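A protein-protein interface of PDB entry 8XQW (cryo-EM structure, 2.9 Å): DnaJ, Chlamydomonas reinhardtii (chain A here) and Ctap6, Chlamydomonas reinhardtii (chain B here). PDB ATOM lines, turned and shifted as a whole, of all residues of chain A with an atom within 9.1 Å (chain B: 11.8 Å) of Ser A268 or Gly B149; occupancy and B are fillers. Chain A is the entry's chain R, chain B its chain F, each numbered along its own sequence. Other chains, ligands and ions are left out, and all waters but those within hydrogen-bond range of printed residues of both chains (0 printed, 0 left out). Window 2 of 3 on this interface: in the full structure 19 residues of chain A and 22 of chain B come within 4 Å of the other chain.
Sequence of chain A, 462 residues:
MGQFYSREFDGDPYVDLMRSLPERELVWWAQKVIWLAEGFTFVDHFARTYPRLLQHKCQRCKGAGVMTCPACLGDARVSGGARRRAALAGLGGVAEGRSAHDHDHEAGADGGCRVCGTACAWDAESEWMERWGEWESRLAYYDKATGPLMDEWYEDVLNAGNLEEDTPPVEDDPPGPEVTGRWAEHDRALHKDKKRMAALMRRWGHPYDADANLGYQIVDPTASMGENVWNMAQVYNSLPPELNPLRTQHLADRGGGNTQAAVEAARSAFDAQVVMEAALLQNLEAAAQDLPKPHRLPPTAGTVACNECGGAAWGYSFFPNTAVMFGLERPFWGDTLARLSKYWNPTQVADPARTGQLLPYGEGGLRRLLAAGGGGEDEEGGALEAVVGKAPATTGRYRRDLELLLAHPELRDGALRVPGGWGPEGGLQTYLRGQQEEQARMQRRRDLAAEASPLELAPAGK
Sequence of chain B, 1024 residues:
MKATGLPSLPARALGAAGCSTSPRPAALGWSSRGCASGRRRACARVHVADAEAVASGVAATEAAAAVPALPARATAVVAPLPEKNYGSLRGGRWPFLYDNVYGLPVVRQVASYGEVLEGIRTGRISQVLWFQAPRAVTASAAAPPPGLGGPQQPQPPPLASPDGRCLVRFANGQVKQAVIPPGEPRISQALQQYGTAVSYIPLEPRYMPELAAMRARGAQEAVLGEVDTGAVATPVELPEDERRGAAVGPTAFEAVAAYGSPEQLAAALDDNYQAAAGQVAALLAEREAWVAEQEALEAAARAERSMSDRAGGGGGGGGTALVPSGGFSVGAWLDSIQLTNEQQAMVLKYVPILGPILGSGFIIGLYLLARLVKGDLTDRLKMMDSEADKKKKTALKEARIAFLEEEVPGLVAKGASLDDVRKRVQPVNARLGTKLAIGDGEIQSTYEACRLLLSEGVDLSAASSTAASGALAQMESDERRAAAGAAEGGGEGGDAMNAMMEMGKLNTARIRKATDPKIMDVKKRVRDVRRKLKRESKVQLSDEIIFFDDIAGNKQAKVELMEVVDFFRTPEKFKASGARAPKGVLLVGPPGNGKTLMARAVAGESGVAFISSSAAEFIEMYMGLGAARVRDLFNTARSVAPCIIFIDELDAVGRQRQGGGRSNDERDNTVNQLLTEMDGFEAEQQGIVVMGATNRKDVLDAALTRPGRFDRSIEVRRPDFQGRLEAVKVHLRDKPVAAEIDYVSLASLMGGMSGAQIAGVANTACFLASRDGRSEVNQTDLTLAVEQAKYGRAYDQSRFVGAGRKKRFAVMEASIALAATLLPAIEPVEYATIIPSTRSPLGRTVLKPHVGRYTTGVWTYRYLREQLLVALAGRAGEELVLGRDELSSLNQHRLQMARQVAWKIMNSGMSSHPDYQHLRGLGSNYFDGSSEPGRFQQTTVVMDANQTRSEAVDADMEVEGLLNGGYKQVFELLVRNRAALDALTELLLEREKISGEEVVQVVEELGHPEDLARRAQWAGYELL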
ATOM      1  N   ARG A 138       0.551 -31.284 -18.199  1.00  0.00           N
ATOM      2  CA  ARG A 138       0.311 -29.853 -18.031  1.00  0.00           C
ATOM      3  C   ARG A 138       1.304 -29.023 -18.828  1.00  0.00           C
ATOM      4  O   ARG A 138       0.993 -27.908 -19.248  1.00  0.00           O
ATOM      5  CB  ARG A 138       0.376 -29.466 -16.560  1.00  0.00           C
ATOM      6  CG  ARG A 138      -0.802 -29.928 -15.766  1.00  0.00           C
ATOM      7  CD  ARG A 138      -0.691 -29.502 -14.328  1.00  0.00           C
ATOM      8  NE  ARG A 138      -1.458 -30.389 -13.464  1.00  0.00           N
ATOM      9  CZ  ARG A 138      -2.739 -30.211 -13.167  1.00  0.00           C
ATOM     10  NH1 ARG A 138      -3.396 -29.173 -13.660  1.00  0.00           N
ATOM     11  NH2 ARG A 138      -3.366 -31.068 -12.377  1.00  0.00           N
ATOM     12  N   LEU A 239      -3.634 -20.555 -17.549  1.00  0.00           N
ATOM     13  CA  LEU A 239      -4.126 -21.787 -16.968  1.00  0.00           C
ATOM     14  C   LEU A 239      -4.461 -22.783 -18.068  1.00  0.00           C
ATOM     15  O   LEU A 239      -4.938 -22.392 -19.136  1.00  0.00           O
ATOM     16  CB  LEU A 239      -5.369 -21.527 -16.118  1.00  0.00           C
ATOM     17  CG  LEU A 239      -5.105 -21.016 -14.710  1.00  0.00           C
ATOM     18  CD1 LEU A 239      -6.343 -20.362 -14.148  1.00  0.00           C
ATOM     19  CD2 LEU A 239      -4.652 -22.155 -13.824  1.00  0.00           C
ATOM     20  N   LEU A 243      -8.064 -26.615 -15.552  1.00  0.00           N
ATOM     21  CA  LEU A 243      -8.250 -25.764 -14.386  1.00  0.00           C
ATOM     22  C   LEU A 243      -8.942 -24.455 -14.717  1.00  0.00           C
ATOM     23  O   LEU A 243      -9.236 -23.678 -13.805  1.00  0.00           O
ATOM     24  CB  LEU A 243      -6.901 -25.476 -13.720  1.00  0.00           C
ATOM     25  CG  LEU A 243      -5.955 -26.654 -13.495  1.00  0.00           C
ATOM     26  CD1 LEU A 243      -4.530 -26.179 -13.562  1.00  0.00           C
ATOM     27  CD2 LEU A 243      -6.230 -27.303 -12.163  1.00  0.00           C
ATOM     28  N   ALA A 261     -15.765 -27.257  -6.863  1.00  0.00           N
ATOM     29  CA  ALA A 261     -14.932 -27.239  -5.670  1.00  0.00           C
ATOM     30  C   ALA A 261     -13.629 -27.988  -5.898  1.00  0.00           C
ATOM     31  O   ALA A 261     -12.551 -27.480  -5.577  1.00  0.00           O
ATOM     32  CB  ALA A 261     -15.689 -27.841  -4.485  1.00  0.00           C
ATOM     33  N   ALA A 262     -13.712 -29.186  -6.472  1.00  0.00           N
ATOM     34  CA  ALA A 262     -12.525 -29.969  -6.770  1.00  0.00           C
ATOM     35  C   ALA A 262     -11.738 -29.427  -7.953  1.00  0.00           C
ATOM     36  O   ALA A 262     -10.829 -30.111  -8.430  1.00  0.00           O
ATOM     37  CB  ALA A 262     -12.904 -31.425  -7.037  1.00  0.00           C
ATOM     38  N   VAL A 263     -12.073 -28.242  -8.446  1.00  0.00           N
ATOM     39  CA  VAL A 263     -11.258 -27.585  -9.459  1.00  0.00           C
ATOM     40  C   VAL A 263     -10.532 -26.383  -8.878  1.00  0.00           C
ATOM     41  O   VAL A 263      -9.345 -26.174  -9.148  1.00  0.00           O
ATOM     42  CB  VAL A 263     -12.128 -27.192 -10.665  1.00  0.00           C
ATOM     43  CG1 VAL A 263     -11.456 -26.100 -11.467  1.00  0.00           C
ATOM     44  CG2 VAL A 263     -12.377 -28.402 -11.532  1.00  0.00           C
ATOM     45  N   GLU A 264     -11.214 -25.587  -8.060  1.00  0.00           N
ATOM     46  CA  GLU A 264     -10.513 -24.548  -7.324  1.00  0.00           C
ATOM     47  C   GLU A 264      -9.648 -25.131  -6.217  1.00  0.00           C
ATOM     48  O   GLU A 264      -8.785 -24.427  -5.686  1.00  0.00           O
ATOM     49  CB  GLU A 264     -11.509 -23.551  -6.742  1.00  0.00           C
ATOM     50  CG  GLU A 264     -12.455 -24.152  -5.724  1.00  0.00           C
ATOM     51  CD  GLU A 264     -11.888 -24.137  -4.320  1.00  0.00           C
ATOM     52  OE1 GLU A 264     -11.695 -23.033  -3.769  1.00  0.00           O
ATOM     53  OE2 GLU A 264     -11.625 -25.227  -3.771  1.00  0.00           O
ATOM     54  N   ALA A 265      -9.864 -26.393  -5.853  1.00  0.00           N
ATOM     55  CA  ALA A 265      -8.988 -27.042  -4.889  1.00  0.00           C
ATOM     56  C   ALA A 265      -7.838 -27.762  -5.571  1.00  0.00           C
ATOM     57  O   ALA A 265      -6.994 -28.349  -4.891  1.00  0.00           O
ATOM     58  CB  ALA A 265      -9.778 -28.020  -4.026  1.00  0.00           C
ATOM     59  N   ALA A 266      -7.805 -27.760  -6.901  1.00  0.00           N
ATOM     60  CA  ALA A 266      -6.631 -28.245  -7.607  1.00  0.00           C
ATOM     61  C   ALA A 266      -5.799 -27.098  -8.149  1.00  0.00           C
ATOM     62  O   ALA A 266      -4.563 -27.174  -8.149  1.00  0.00           O
ATOM     63  CB  ALA A 266      -7.040 -29.175  -8.743  1.00  0.00           C
ATOM     64  N   ARG A 267      -6.453 -26.032  -8.608  1.00  0.00           N
ATOM     65  CA  ARG A 267      -5.717 -24.864  -9.076  1.00  0.00           C
ATOM     66  C   ARG A 267      -4.886 -24.259  -7.951  1.00  0.00           C
ATOM     67  O   ARG A 267      -3.786 -23.740  -8.183  1.00  0.00           O
ATOM     68  CB  ARG A 267      -6.692 -23.843  -9.651  1.00  0.00           C
ATOM     69  CG  ARG A 267      -6.132 -22.458  -9.817  1.00  0.00           C
ATOM     70  CD  ARG A 267      -7.204 -21.497 -10.284  1.00  0.00           C
ATOM     71  NE  ARG A 267      -8.505 -21.770  -9.677  1.00  0.00           N
ATOM     72  CZ  ARG A 267      -9.583 -22.160 -10.353  1.00  0.00           C
ATOM     73  NH1 ARG A 267      -9.526 -22.335 -11.666  1.00  0.00           N
ATOM     74  NH2 ARG A 267     -10.725 -22.381  -9.718  1.00  0.00           N
ATOM     75  N   SER A 268      -5.380 -24.348  -6.718  1.00  0.00           N
ATOM     76  CA  SER A 268      -4.618 -23.853  -5.579  1.00  0.00           C
ATOM     77  C   SER A 268      -3.326 -24.635  -5.390  1.00  0.00           C
ATOM     78  O   SER A 268      -2.256 -24.041  -5.214  1.00  0.00           O
ATOM     79  CB  SER A 268      -5.470 -23.920  -4.318  1.00  0.00           C
ATOM     80  OG  SER A 268      -6.666 -23.187  -4.489  1.00  0.00           O
ATOM     81  N   ALA A 269      -3.405 -25.965  -5.404  1.00  0.00           N
ATOM     82  CA  ALA A 269      -2.198 -26.768  -5.289  1.00  0.00           C
ATOM     83  C   ALA A 269      -1.242 -26.476  -6.432  1.00  0.00           C
ATOM     84  O   ALA A 269      -0.020 -26.432  -6.239  1.00  0.00           O
ATOM     85  CB  ALA A 269      -2.553 -28.249  -5.253  1.00  0.00           C
ATOM     86  N   PHE A 270      -1.782 -26.255  -7.627  1.00  0.00           N
ATOM     87  CA  PHE A 270      -0.939 -25.919  -8.768  1.00  0.00           C
ATOM     88  C   PHE A 270      -0.137 -24.648  -8.509  1.00  0.00           C
ATOM     89  O   PHE A 270       1.090 -24.610  -8.697  1.00  0.00           O
ATOM     90  CB  PHE A 270      -1.818 -25.770 -10.002  1.00  0.00           C
ATOM     91  CG  PHE A 270      -1.077 -25.393 -11.230  1.00  0.00           C
ATOM     92  CD1 PHE A 270      -0.363 -26.333 -11.927  1.00  0.00           C
ATOM     93  CD2 PHE A 270      -1.116 -24.104 -11.699  1.00  0.00           C
ATOM     94  CE1 PHE A 270       0.303 -25.994 -13.062  1.00  0.00           C
ATOM     95  CE2 PHE A 270      -0.445 -23.759 -12.831  1.00  0.00           C
ATOM     96  CZ  PHE A 270       0.264 -24.706 -13.514  1.00  0.00           C
ATOM     97  N   ASP A 271      -0.808 -23.593  -8.060  1.00  0.00           N
ATOM     98  CA  ASP A 271      -0.104 -22.333  -7.853  1.00  0.00           C
ATOM     99  C   ASP A 271       0.872 -22.420  -6.690  1.00  0.00           C
ATOM    100  O   ASP A 271       1.918 -21.759  -6.699  1.00  0.00           O
ATOM    101  CB  ASP A 271      -1.107 -21.210  -7.648  1.00  0.00           C
ATOM    102  CG  ASP A 271      -1.874 -20.904  -8.902  1.00  0.00           C
ATOM    103  OD1 ASP A 271      -1.470 -21.415  -9.961  1.00  0.00           O
ATOM    104  OD2 ASP A 271      -2.874 -20.161  -8.835  1.00  0.00           O
ATOM    105  N   ALA A 272       0.561 -23.238  -5.686  1.00  0.00           N
ATOM    106  CA  ALA A 272       1.527 -23.459  -4.619  1.00  0.00           C
ATOM    107  C   ALA A 272       2.796 -24.109  -5.151  1.00  0.00           C
ATOM    108  O   ALA A 272       3.906 -23.718  -4.774  1.00  0.00           O
ATOM    109  CB  ALA A 272       0.914 -24.311  -3.518  1.00  0.00           C
ATOM    110  N   GLN A 273       2.654 -25.102  -6.029  1.00  0.00           N
ATOM    111  CA  GLN A 273       3.839 -25.701  -6.635  1.00  0.00           C
ATOM    112  C   GLN A 273       4.656 -24.665  -7.388  1.00  0.00           C
ATOM    113  O   GLN A 273       5.890 -24.658  -7.315  1.00  0.00           O
ATOM    114  CB  GLN A 273       3.446 -26.832  -7.574  1.00  0.00           C
ATOM    115  CG  GLN A 273       2.642 -27.922  -6.935  1.00  0.00           C
ATOM    116  CD  GLN A 273       3.487 -28.894  -6.169  1.00  0.00           C
ATOM    117  OE1 GLN A 273       3.444 -28.933  -4.947  1.00  0.00           O
ATOM    118  NE2 GLN A 273       4.258 -29.696  -6.883  1.00  0.00           N
ATOM    119  N   VAL A 274       3.993 -23.776  -8.119  1.00  0.00           N
ATOM    120  CA  VAL A 274       4.754 -22.803  -8.901  1.00  0.00           C
ATOM    121  C   VAL A 274       5.522 -21.845  -7.994  1.00  0.00           C
ATOM    122  O   VAL A 274       6.703 -21.541  -8.234  1.00  0.00           O
ATOM    123  CB  VAL A 274       3.828 -22.052  -9.865  1.00  0.00           C
ATOM    124  CG1 VAL A 274       4.461 -20.762 -10.286  1.00  0.00           C
ATOM    125  CG2 VAL A 274       3.561 -22.909 -11.067  1.00  0.00           C
ATOM    126  N   VAL A 275       4.878 -21.347  -6.940  1.00  0.00           N
ATOM    127  CA  VAL A 275       5.588 -20.433  -6.052  1.00  0.00           C
ATOM    128  C   VAL A 275       6.746 -21.137  -5.358  1.00  0.00           C
ATOM    129  O   VAL A 275       7.820 -20.547  -5.169  1.00  0.00           O
ATOM    130  CB  VAL A 275       4.625 -19.806  -5.036  1.00  0.00           C
ATOM    131  CG1 VAL A 275       5.352 -18.817  -4.182  1.00  0.00           C
ATOM    132  CG2 VAL A 275       3.504 -19.122  -5.757  1.00  0.00           C
ATOM    133  N   MET A 276       6.565 -22.401  -4.974  1.00  0.00           N
ATOM    134  CA  MET A 276       7.670 -23.143  -4.381  1.00  0.00           C
ATOM    135  C   MET A 276       8.836 -23.250  -5.345  1.00  0.00           C
ATOM    136  O   MET A 276       9.997 -23.169  -4.933  1.00  0.00           O
ATOM    137  CB  MET A 276       7.209 -24.529  -3.964  1.00  0.00           C
ATOM    138  CG  MET A 276       6.752 -24.586  -2.543  1.00  0.00           C
ATOM    139  SD  MET A 276       7.946 -23.819  -1.444  1.00  0.00           S
ATOM    140  CE  MET A 276       9.225 -25.063  -1.432  1.00  0.00           C
ATOM    141  N   ALA B 143       4.557 -30.605   2.395  1.00  0.00           N
ATOM    142  CA  ALA B 143       3.753 -29.874   1.428  1.00  0.00           C
ATOM    143  C   ALA B 143       4.186 -28.419   1.452  1.00  0.00           C
ATOM    144  O   ALA B 143       4.811 -27.977   2.421  1.00  0.00           O
ATOM    145  CB  ALA B 143       2.258 -30.000   1.741  1.00  0.00           C
ATOM    146  N   PRO B 144       3.886 -27.656   0.405  1.00  0.00           N
ATOM    147  CA  PRO B 144       4.233 -26.237   0.399  1.00  0.00           C
ATOM    148  C   PRO B 144       3.663 -25.531   1.613  1.00  0.00           C
ATOM    149  O   PRO B 144       2.639 -25.957   2.164  1.00  0.00           O
ATOM    150  CB  PRO B 144       3.594 -25.733  -0.898  1.00  0.00           C
ATOM    151  CG  PRO B 144       3.652 -26.898  -1.783  1.00  0.00           C
ATOM    152  CD  PRO B 144       3.405 -28.095  -0.915  1.00  0.00           C
ATOM    153  N   PRO B 145       4.303 -24.454   2.062  1.00  0.00           N
ATOM    154  CA  PRO B 145       3.955 -23.886   3.358  1.00  0.00           C
ATOM    155  C   PRO B 145       2.524 -23.422   3.385  1.00  0.00           C
ATOM    156  O   PRO B 145       1.964 -22.986   2.358  1.00  0.00           O
ATOM    157  CB  PRO B 145       4.930 -22.708   3.494  1.00  0.00           C
ATOM    158  CG  PRO B 145       6.052 -23.053   2.622  1.00  0.00           C
ATOM    159  CD  PRO B 145       5.473 -23.793   1.471  1.00  0.00           C
ATOM    160  N   PRO B 146       1.872 -23.489   4.534  1.00  0.00           N
ATOM    161  CA  PRO B 146       0.545 -22.896   4.667  1.00  0.00           C
ATOM    162  C   PRO B 146       0.640 -21.387   4.649  1.00  0.00           C
ATOM    163  O   PRO B 146       1.084 -20.769   5.618  1.00  0.00           O
ATOM    164  CB  PRO B 146       0.062 -23.417   6.022  1.00  0.00           C
ATOM    165  CG  PRO B 146       1.306 -23.671   6.770  1.00  0.00           C
ATOM    166  CD  PRO B 146       2.306 -24.146   5.775  1.00  0.00           C
ATOM    167  N   GLY B 147       0.217 -20.781   3.554  1.00  0.00           N
ATOM    168  CA  GLY B 147       0.464 -19.375   3.349  1.00  0.00           C
ATOM    169  C   GLY B 147       0.731 -19.153   1.885  1.00  0.00           C
ATOM    170  O   GLY B 147       0.701 -18.025   1.392  1.00  0.00           O
ATOM    171  N   LEU B 148       1.015 -20.247   1.187  1.00  0.00           N
ATOM    172  CA  LEU B 148       0.941 -20.260  -0.261  1.00  0.00           C
ATOM    173  C   LEU B 148      -0.473 -20.507  -0.755  1.00  0.00           C
ATOM    174  O   LEU B 148      -0.713 -20.422  -1.961  1.00  0.00           O
ATOM    175  CB  LEU B 148       1.881 -21.320  -0.828  1.00  0.00           C
ATOM    176  CG  LEU B 148       3.362 -21.047  -0.600  1.00  0.00           C
ATOM    177  CD1 LEU B 148       4.207 -22.027  -1.359  1.00  0.00           C
ATOM    178  CD2 LEU B 148       3.682 -19.653  -1.041  1.00  0.00           C
ATOM    179  N   GLY B 149      -1.404 -20.821   0.137  1.00  0.00           N
ATOM    180  CA  GLY B 149      -2.804 -20.885  -0.208  1.00  0.00           C
ATOM    181  C   GLY B 149      -3.304 -22.212  -0.719  1.00  0.00           C
ATOM    182  O   GLY B 149      -4.383 -22.255  -1.315  1.00  0.00           O
ATOM    183  N   GLY B 150      -2.573 -23.293  -0.508  1.00  0.00           N
ATOM    184  CA  GLY B 150      -3.010 -24.582  -0.984  1.00  0.00           C
ATOM    185  C   GLY B 150      -4.125 -25.160  -0.141  1.00  0.00           C
ATOM    186  O   GLY B 150      -4.602 -24.539   0.810  1.00  0.00           O
ATOM    187  N   PRO B 151      -4.566 -26.366  -0.481  1.00  0.00           N
ATOM    188  CA  PRO B 151      -5.549 -27.046   0.359  1.00  0.00           C
ATOM    189  C   PRO B 151      -4.940 -27.434   1.694  1.00  0.00           C
ATOM    190  O   PRO B 151      -3.744 -27.697   1.810  1.00  0.00           O
ATOM    191  CB  PRO B 151      -5.927 -28.279  -0.461  1.00  0.00           C
ATOM    192  CG  PRO B 151      -4.770 -28.506  -1.346  1.00  0.00           C
ATOM    193  CD  PRO B 151      -4.225 -27.154  -1.674  1.00  0.00           C
ATOM    194  N   GLN B 152      -5.789 -27.472   2.711  1.00  0.00           N
ATOM    195  CA  GLN B 152      -5.338 -27.723   4.070  1.00  0.00           C
ATOM    196  C   GLN B 152      -4.833 -29.152   4.217  1.00  0.00           C
ATOM    197  O   GLN B 152      -5.596 -30.106   4.056  1.00  0.00           O
ATOM    198  CB  GLN B 152      -6.479 -27.468   5.045  1.00  0.00           C
ATOM    199  CG  GLN B 152      -6.080 -27.529   6.486  1.00  0.00           C
ATOM    200  CD  GLN B 152      -6.838 -26.534   7.319  1.00  0.00           C
ATOM    201  OE1 GLN B 152      -7.662 -26.904   8.147  1.00  0.00           O
ATOM    202  NE2 GLN B 152      -6.573 -25.256   7.098  1.00  0.00           N
ATOM    203  N   GLN B 153      -3.560 -29.293   4.519  1.00  0.00           N
ATOM    204  CA  GLN B 153      -2.976 -30.601   4.755  1.00  0.00           C
ATOM    205  C   GLN B 153      -3.404 -31.118   6.116  1.00  0.00           C
ATOM    206  O   GLN B 153      -3.675 -30.335   7.026  1.00  0.00           O
ATOM    207  CB  GLN B 153      -1.456 -30.516   4.673  1.00  0.00           C
ATOM    208  CG  GLN B 153      -0.952 -29.822   3.436  1.00  0.00           C
ATOM    209  CD  GLN B 153      -1.432 -30.477   2.160  1.00  0.00           C
ATOM    210  OE1 GLN B 153      -1.828 -29.798   1.215  1.00  0.00           O
ATOM    211  NE2 GLN B 153      -1.391 -31.799   2.122  1.00  0.00           N
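OG of Ser A268 sits at hydrogen-bond distance from O of Glu A264, 2.7 Å away.
The side-chain amide oxygen (OE1) of Gln B153 lies close to the backbone carbonyl oxygen (O) of Pro B151, 2.9 Å away.
No residue of chain B comes within 4 Å of Ala A265.
No residue of chain B comes within 4 Å of Arg A267.
Ser A268 touches one residue of chain B.
Printed residues of chain B within 4 Å of Gln A273: Pro B144.
Printed residues of chain B within 4 Å of Met A276: Pro B144, Pro B145 and Leu B148.
Of the printed residues of chain A, Pro B144 touches Gln A273 (3.8 Å) and Met A276 (3.7 Å).
Of the printed residues of chain A, Pro B145 touches Met A276 (3.8 Å).
Pro B146 touches none of the printed residues of chain A.
No residue of chain A comes within 4 Å of Gly B147.
Gly B149 touches just one residue of chain A: Ser A268 (3.6 Å).
Gly B150 touches none of the printed residues of chain A.
Printed residues of chain A within 4 Å of Pro B151: Ala A269.
The nearest residue of chain A that does not touch Gly B149 is Ala A272 (5.5 Å).
The nearest printed residue of chain A that does not touch Leu B148 is Ser A268 (5.1 Å).
Gly B149 touches Ser A268.
Ala A269 touches Pro B151.
CD1 of Leu B148 touches O of Ala A272, 3.8 Å away.
CG of Pro B144 touches OE1 of Gln A273, 3.8 Å away.
CD2 of Leu B148 touches CG1 of Val A275 (3.7 Å).
CG of Met A276 touches CB of Pro B144, 3.7 Å away.
SD of Met A276 touches CD of Pro B145, at 3.8 Å.
CG of Met A276 touches CD1 of Leu B148, 3.8 Å away.
Printed residues of chain B that touch a printed residue of chain A: Pro B144, Pro B145, Leu B148, Gly B149 and Pro B151.
Hydrophobic or aromatic side chains of chain B within 4 Å of the printed part of chain A: Pro B144, Pro B145, Leu B148 and Pro B151.
Hydrophobic or aromatic side chains of chain A within 4 Å of the printed part of chain B: Val A275 and Met A276.
Among the printed residues, no Asp or Glu carboxylate lies within 4 Å of a Lys or Arg side-chain nitrogen of the other chain.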
